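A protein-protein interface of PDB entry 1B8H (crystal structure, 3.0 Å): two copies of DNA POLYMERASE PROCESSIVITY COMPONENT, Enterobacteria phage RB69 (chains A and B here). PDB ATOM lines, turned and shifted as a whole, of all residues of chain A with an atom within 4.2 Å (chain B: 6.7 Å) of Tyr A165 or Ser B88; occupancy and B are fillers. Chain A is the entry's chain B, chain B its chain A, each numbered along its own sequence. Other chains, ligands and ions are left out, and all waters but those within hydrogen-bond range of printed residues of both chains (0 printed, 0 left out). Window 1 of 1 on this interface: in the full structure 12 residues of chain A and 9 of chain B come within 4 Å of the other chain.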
ATOM      1  N   GLN A 125      -4.560  12.903 -10.954  1.00  0.00           N
ATOM      2  CA  GLN A 125      -4.852  13.471 -12.264  1.00  0.00           C
ATOM      3  C   GLN A 125      -6.325  13.318 -12.622  1.00  0.00           C
ATOM      4  O   GLN A 125      -6.922  14.221 -13.187  1.00  0.00           O
ATOM      5  CB  GLN A 125      -4.025  12.824 -13.373  1.00  0.00           C
ATOM      6  CG  GLN A 125      -4.252  13.502 -14.729  1.00  0.00           C
ATOM      7  CD  GLN A 125      -3.659  12.742 -15.906  1.00  0.00           C
ATOM      8  OE1 GLN A 125      -4.197  11.721 -16.347  1.00  0.00           O
ATOM      9  NE2 GLN A 125      -2.542  13.243 -16.421  1.00  0.00           N
ATOM     10  N   LEU A 126      -6.899  12.158 -12.313  1.00  0.00           N
ATOM     11  CA  LEU A 126      -8.308  11.879 -12.593  1.00  0.00           C
ATOM     12  C   LEU A 126      -9.216  12.947 -11.978  1.00  0.00           C
ATOM     13  O   LEU A 126     -10.067  13.517 -12.660  1.00  0.00           O
ATOM     14  CB  LEU A 126      -8.678  10.489 -12.049  1.00  0.00           C
ATOM     15  CG  LEU A 126     -10.136   9.988 -12.096  1.00  0.00           C
ATOM     16  CD1 LEU A 126     -10.706  10.069 -13.504  1.00  0.00           C
ATOM     17  CD2 LEU A 126     -10.185   8.549 -11.588  1.00  0.00           C
ATOM     18  N   ILE A 135     -16.398  16.503 -15.763  1.00  0.00           N
ATOM     19  CA  ILE A 135     -16.688  15.088 -15.840  1.00  0.00           C
ATOM     20  C   ILE A 135     -17.495  14.710 -14.606  1.00  0.00           C
ATOM     21  O   ILE A 135     -16.960  14.677 -13.501  1.00  0.00           O
ATOM     22  CB  ILE A 135     -15.368  14.268 -15.923  1.00  0.00           C
ATOM     23  CG1 ILE A 135     -14.689  14.551 -17.275  1.00  0.00           C
ATOM     24  CG2 ILE A 135     -15.650  12.777 -15.726  1.00  0.00           C
ATOM     25  CD1 ILE A 135     -13.350  13.917 -17.452  1.00  0.00           C
ATOM     26  N   ILE A 149     -10.401   3.568 -17.403  1.00  0.00           N
ATOM     27  CA  ILE A 149     -11.439   4.417 -16.839  1.00  0.00           C
ATOM     28  C   ILE A 149     -11.778   5.440 -17.899  1.00  0.00           C
ATOM     29  O   ILE A 149     -10.882   6.081 -18.444  1.00  0.00           O
ATOM     30  CB  ILE A 149     -10.945   5.147 -15.587  1.00  0.00           C
ATOM     31  CG1 ILE A 149     -10.605   4.119 -14.510  1.00  0.00           C
ATOM     32  CG2 ILE A 149     -12.006   6.134 -15.097  1.00  0.00           C
ATOM     33  CD1 ILE A 149      -9.937   4.705 -13.317  1.00  0.00           C
ATOM     34  N   ASN A 150     -13.062   5.572 -18.212  1.00  0.00           N
ATOM     35  CA  ASN A 150     -13.500   6.530 -19.217  1.00  0.00           C
ATOM     36  C   ASN A 150     -14.369   7.574 -18.542  1.00  0.00           C
ATOM     37  O   ASN A 150     -15.355   7.230 -17.887  1.00  0.00           O
ATOM     38  CB  ASN A 150     -14.316   5.843 -20.316  1.00  0.00           C
ATOM     39  CG  ASN A 150     -13.486   4.914 -21.173  1.00  0.00           C
ATOM     40  OD1 ASN A 150     -12.408   5.271 -21.638  1.00  0.00           O
ATOM     41  ND2 ASN A 150     -13.999   3.715 -21.406  1.00  0.00           N
ATOM     42  N   GLY A 151     -13.994   8.844 -18.700  1.00  0.00           N
ATOM     43  CA  GLY A 151     -14.750   9.930 -18.093  1.00  0.00           C
ATOM     44  C   GLY A 151     -15.696  10.650 -19.040  1.00  0.00           C
ATOM     45  O   GLY A 151     -15.299  11.092 -20.116  1.00  0.00           O
ATOM     46  N   PRO A 163     -16.432   9.883 -24.504  1.00  0.00           N
ATOM     47  CA  PRO A 163     -15.435  10.102 -23.450  1.00  0.00           C
ATOM     48  C   PRO A 163     -14.545  11.339 -23.585  1.00  0.00           C
ATOM     49  O   PRO A 163     -13.964  11.590 -24.643  1.00  0.00           O
ATOM     50  CB  PRO A 163     -14.628   8.803 -23.463  1.00  0.00           C
ATOM     51  CG  PRO A 163     -14.780   8.313 -24.846  1.00  0.00           C
ATOM     52  CD  PRO A 163     -16.239   8.552 -25.104  1.00  0.00           C
ATOM     53  N   LYS A 164     -14.428  12.087 -22.489  1.00  0.00           N
ATOM     54  CA  LYS A 164     -13.615  13.298 -22.440  1.00  0.00           C
ATOM     55  C   LYS A 164     -12.245  12.999 -21.827  1.00  0.00           C
ATOM     56  O   LYS A 164     -11.271  13.700 -22.068  1.00  0.00           O
ATOM     57  CB  LYS A 164     -14.349  14.379 -21.634  1.00  0.00           C
ATOM     58  CG  LYS A 164     -15.871  14.331 -21.799  1.00  0.00           C
ATOM     59  CD  LYS A 164     -16.560  15.580 -21.259  1.00  0.00           C
ATOM     60  CE  LYS A 164     -16.476  16.744 -22.238  1.00  0.00           C
ATOM     61  NZ  LYS A 164     -16.985  18.012 -21.636  1.00  0.00           N
ATOM     62  N   TYR A 165     -12.167  11.939 -21.042  1.00  0.00           N
ATOM     63  CA  TYR A 165     -10.903  11.544 -20.422  1.00  0.00           C
ATOM     64  C   TYR A 165     -10.796  10.019 -20.485  1.00  0.00           C
ATOM     65  O   TYR A 165     -11.819   9.333 -20.540  1.00  0.00           O
ATOM     66  CB  TYR A 165     -10.871  12.020 -18.970  1.00  0.00           C
ATOM     67  CG  TYR A 165      -9.699  11.520 -18.167  1.00  0.00           C
ATOM     68  CD1 TYR A 165      -8.392  11.886 -18.490  1.00  0.00           C
ATOM     69  CD2 TYR A 165      -9.899  10.716 -17.058  1.00  0.00           C
ATOM     70  CE1 TYR A 165      -7.309  11.462 -17.713  1.00  0.00           C
ATOM     71  CE2 TYR A 165      -8.836  10.285 -16.277  1.00  0.00           C
ATOM     72  CZ  TYR A 165      -7.541  10.660 -16.602  1.00  0.00           C
ATOM     73  OH  TYR A 165      -6.496  10.244 -15.806  1.00  0.00           O
ATOM     74  N   SER A 166      -9.568   9.499 -20.486  1.00  0.00           N
ATOM     75  CA  SER A 166      -9.373   8.057 -20.559  1.00  0.00           C
ATOM     76  C   SER A 166      -8.045   7.590 -19.954  1.00  0.00           C
ATOM     77  O   SER A 166      -6.972   7.870 -20.489  1.00  0.00           O
ATOM     78  CB  SER A 166      -9.476   7.591 -22.011  1.00  0.00           C
ATOM     79  OG  SER A 166      -9.813   6.225 -22.077  1.00  0.00           O
ATOM     80  N   LEU A 167      -8.152   6.877 -18.833  1.00  0.00           N
ATOM     81  CA  LEU A 167      -7.011   6.371 -18.100  1.00  0.00           C
ATOM     82  C   LEU A 167      -6.900   4.854 -18.113  1.00  0.00           C
ATOM     83  O   LEU A 167      -7.857   4.132 -17.789  1.00  0.00           O
ATOM     84  CB  LEU A 167      -7.056   6.841 -16.649  1.00  0.00           C
ATOM     85  CG  LEU A 167      -5.981   6.279 -15.730  1.00  0.00           C
ATOM     86  CD1 LEU A 167      -4.587   6.688 -16.238  1.00  0.00           C
ATOM     87  CD2 LEU A 167      -6.209   6.746 -14.284  1.00  0.00           C
ATOM     88  N   VAL B  67      -1.290  17.520 -16.883  1.00  0.00           N
ATOM     89  CA  VAL B  67      -0.673  16.446 -17.647  1.00  0.00           C
ATOM     90  C   VAL B  67       0.823  16.616 -17.797  1.00  0.00           C
ATOM     91  O   VAL B  67       1.410  17.583 -17.325  1.00  0.00           O
ATOM     92  CB  VAL B  67      -1.281  16.284 -19.075  1.00  0.00           C
ATOM     93  CG1 VAL B  67      -2.699  15.806 -18.976  1.00  0.00           C
ATOM     94  CG2 VAL B  67      -1.206  17.581 -19.837  1.00  0.00           C
ATOM     95  N   LYS B  82      -6.825  16.117 -29.086  1.00  0.00           N
ATOM     96  CA  LYS B  82      -6.374  14.993 -28.265  1.00  0.00           C
ATOM     97  C   LYS B  82      -5.045  15.317 -27.590  1.00  0.00           C
ATOM     98  O   LYS B  82      -4.064  15.608 -28.268  1.00  0.00           O
ATOM     99  CB  LYS B  82      -6.179  13.739 -29.114  1.00  0.00           C
ATOM    100  CG  LYS B  82      -5.434  12.625 -28.381  1.00  0.00           C
ATOM    101  CD  LYS B  82      -5.132  11.456 -29.312  1.00  0.00           C
ATOM    102  CE  LYS B  82      -4.473  10.282 -28.575  1.00  0.00           C
ATOM    103  NZ  LYS B  82      -4.303   9.051 -29.416  1.00  0.00           N
ATOM    104  N   ILE B  83      -5.011  15.270 -26.262  1.00  0.00           N
ATOM    105  CA  ILE B  83      -3.781  15.538 -25.507  1.00  0.00           C
ATOM    106  C   ILE B  83      -3.262  14.172 -25.006  1.00  0.00           C
ATOM    107  O   ILE B  83      -3.731  13.653 -23.984  1.00  0.00           O
ATOM    108  CB  ILE B  83      -4.060  16.511 -24.297  1.00  0.00           C
ATOM    109  CG1 ILE B  83      -4.733  17.794 -24.800  1.00  0.00           C
ATOM    110  CG2 ILE B  83      -2.763  16.902 -23.600  1.00  0.00           C
ATOM    111  CD1 ILE B  83      -5.119  18.738 -23.691  1.00  0.00           C
ATOM    112  N   ALA B  84      -2.312  13.589 -25.735  1.00  0.00           N
ATOM    113  CA  ALA B  84      -1.754  12.283 -25.382  1.00  0.00           C
ATOM    114  C   ALA B  84      -0.787  12.325 -24.214  1.00  0.00           C
ATOM    115  O   ALA B  84       0.238  12.982 -24.294  1.00  0.00           O
ATOM    116  CB  ALA B  84      -1.060  11.691 -26.576  1.00  0.00           C
ATOM    117  N   ASP B  85      -1.105  11.605 -23.142  1.00  0.00           N
ATOM    118  CA  ASP B  85      -0.249  11.562 -21.957  1.00  0.00           C
ATOM    119  C   ASP B  85       0.319  10.156 -21.768  1.00  0.00           C
ATOM    120  O   ASP B  85      -0.079   9.209 -22.455  1.00  0.00           O
ATOM    121  CB  ASP B  85      -1.048  11.970 -20.713  1.00  0.00           C
ATOM    122  CG  ASP B  85      -0.161  12.402 -19.549  1.00  0.00           C
ATOM    123  OD1 ASP B  85       1.074  12.482 -19.703  1.00  0.00           O
ATOM    124  OD2 ASP B  85      -0.713  12.678 -18.469  1.00  0.00           O
ATOM    125  N   THR B  86       1.247  10.039 -20.822  1.00  0.00           N
ATOM    126  CA  THR B  86       1.924   8.784 -20.488  1.00  0.00           C
ATOM    127  C   THR B  86       1.034   7.535 -20.441  1.00  0.00           C
ATOM    128  O   THR B  86       1.291   6.570 -21.166  1.00  0.00           O
ATOM    129  CB  THR B  86       2.659   8.934 -19.137  1.00  0.00           C
ATOM    130  OG1 THR B  86       3.511  10.087 -19.194  1.00  0.00           O
ATOM    131  CG2 THR B  86       3.510   7.705 -18.842  1.00  0.00           C
ATOM    132  N   ARG B  87       0.014   7.544 -19.580  1.00  0.00           N
ATOM    133  CA  ARG B  87      -0.903   6.407 -19.450  1.00  0.00           C
ATOM    134  C   ARG B  87      -2.336   6.863 -19.662  1.00  0.00           C
ATOM    135  O   ARG B  87      -3.272   6.106 -19.391  1.00  0.00           O
ATOM    136  CB  ARG B  87      -0.838   5.771 -18.048  1.00  0.00           C
ATOM    137  CG  ARG B  87       0.440   5.033 -17.676  1.00  0.00           C
ATOM    138  CD  ARG B  87       1.441   5.919 -16.928  1.00  0.00           C
ATOM    139  NE  ARG B  87       1.019   6.261 -15.571  1.00  0.00           N
ATOM    140  CZ  ARG B  87       1.639   7.151 -14.798  1.00  0.00           C
ATOM    141  NH1 ARG B  87       2.715   7.802 -15.237  1.00  0.00           N
ATOM    142  NH2 ARG B  87       1.182   7.387 -13.576  1.00  0.00           N
ATOM    143  N   SER B  88      -2.523   8.094 -20.128  1.00  0.00           N
ATOM    144  CA  SER B  88      -3.873   8.604 -20.313  1.00  0.00           C
ATOM    145  C   SER B  88      -4.059   9.474 -21.538  1.00  0.00           C
ATOM    146  O   SER B  88      -3.095   9.839 -22.218  1.00  0.00           O
ATOM    147  CB  SER B  88      -4.300   9.381 -19.068  1.00  0.00           C
ATOM    148  OG  SER B  88      -3.279  10.262 -18.629  1.00  0.00           O
ATOM    149  N   THR B  89      -5.317   9.803 -21.816  1.00  0.00           N
ATOM    150  CA  THR B  89      -5.653  10.640 -22.958  1.00  0.00           C
ATOM    151  C   THR B  89      -6.727  11.647 -22.559  1.00  0.00           C
ATOM    152  O   THR B  89      -7.766  11.275 -22.009  1.00  0.00           O
ATOM    153  CB  THR B  89      -6.153   9.787 -24.129  1.00  0.00           C
ATOM    154  OG1 THR B  89      -5.290   8.654 -24.285  1.00  0.00           O
ATOM    155  CG2 THR B  89      -6.150  10.595 -25.409  1.00  0.00           C
ATOM    156  N   VAL B  90      -6.448  12.927 -22.815  1.00  0.00           N
ATOM    157  CA  VAL B  90      -7.366  14.022 -22.500  1.00  0.00           C
ATOM    158  C   VAL B  90      -7.930  14.593 -23.790  1.00  0.00           C
ATOM    159  O   VAL B  90      -7.174  14.900 -24.700  1.00  0.00           O
ATOM    160  CB  VAL B  90      -6.645  15.165 -21.743  1.00  0.00           C
ATOM    161  CG1 VAL B  90      -7.520  16.394 -21.702  1.00  0.00           C
ATOM    162  CG2 VAL B  90      -6.345  14.740 -20.330  1.00  0.00           C
ATOM    163  N   TYR B  91      -9.244  14.734 -23.890  1.00  0.00           N
ATOM    164  CA  TYR B  91      -9.796  15.296 -25.113  1.00  0.00           C
ATOM    165  C   TYR B  91     -10.313  16.691 -24.845  1.00  0.00           C
ATOM    166  O   TYR B  91     -10.731  16.999 -23.736  1.00  0.00           O
ATOM    167  CB  TYR B  91     -10.933  14.426 -25.662  1.00  0.00           C
ATOM    168  CG  TYR B  91     -10.508  13.018 -25.992  1.00  0.00           C
ATOM    169  CD1 TYR B  91      -9.907  12.718 -27.205  1.00  0.00           C
ATOM    170  CD2 TYR B  91     -10.606  11.998 -25.054  1.00  0.00           C
ATOM    171  CE1 TYR B  91      -9.404  11.440 -27.470  1.00  0.00           C
ATOM    172  CE2 TYR B  91     -10.106  10.718 -25.312  1.00  0.00           C
ATOM    173  CZ  TYR B  91      -9.500  10.447 -26.518  1.00  0.00           C
ATOM    174  OH  TYR B  91      -8.959   9.197 -26.749  1.00  0.00           O
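The side-chain amide nitrogen (NE2) of Gln A125 is in hydrogen-bond range of the side-chain carboxylate (OD2) of Asp B85.
OG of Ser B88 lies within hydrogen-bond range of OE1 of Gln A125, 2.9 Å away.
O of Ser A166 is in hydrogen-bond range of N of Thr B89, at 2.9 Å.
The backbone carbonyl oxygen (O) of Lys A164 sits at hydrogen-bond distance from the backbone NH (N) of Tyr B91.
No position is printed for both chains.
The backbone NH of Ile B83 sits at hydrogen-bond distance from the backbone carbonyl oxygen of Val B90, 2.7 Å away.
The side-chain hydroxyl of Thr B86 is in hydrogen-bond range of the side-chain carboxylate of Asp B85 (3.5 Å).
The side-chain hydroxyl of Tyr A165 is in hydrogen-bond range of the side-chain amide oxygen of Gln A125 (2.8 Å).
The side-chain amide oxygen of Asn A150 sits at hydrogen-bond distance from the side-chain hydroxyl of Ser A166 (2.8 Å).
N of Lys A164 is in hydrogen-bond range of O of Gly A151, 2.7 Å away.
O of Tyr A165 sits at hydrogen-bond distance from N of Gly A151 (2.9 Å).
Tyr A165 touches just these residues of chain B: Ser B88 (3.9 Å), Thr B89 (3.5 Å) and Val B90 (3.96 Å).
Of the printed residues of chain A, Val B90 touches Lys A164 (3.9 Å) and Tyr A165 (3.96 Å).
Of the printed residues of chain B, Pro A163 touches Tyr B91 (3.4 Å).
Lys B82 touches none of the printed residues of chain A.
Gly A151 touches none of the printed residues of chain B.
The nearest residue of chain B that does not touch Tyr A165 is Tyr B91 (4.3 Å).
Printed residues of chain B that touch a printed residue of chain A: Val B67, Asp B85, Arg B87, Ser B88, Thr B89, Val B90 and Tyr B91.
Printed residues of chain A that touch a printed residue of chain B: Gln A125, Pro A163, Lys A164, Tyr A165, Ser A166 and Leu A167.
Hydrophobic or aromatic side chains of chain A that line the printed part of chain B: Tyr A165 and Leu A167.
Val B67 touches Gln A125.
O of Pro A163 touches CD2 of Tyr B91, at 3.4 Å.
Val B90 touches Lys A164 (C to O, 3.9 Å).
Tyr A165 touches Ser B88.
O of Thr B89 touches CA of Tyr A165 (3.5 Å).
CD1 of Tyr A165 touches CG2 of Val B90, at 3.96 Å.
Ser B88 touches Ser A166.
CD1 of Leu A167 touches O of Arg B87 (3.5 Å).
CB of Ser B88 touches CD1 of Leu A167, 3.9 Å away.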
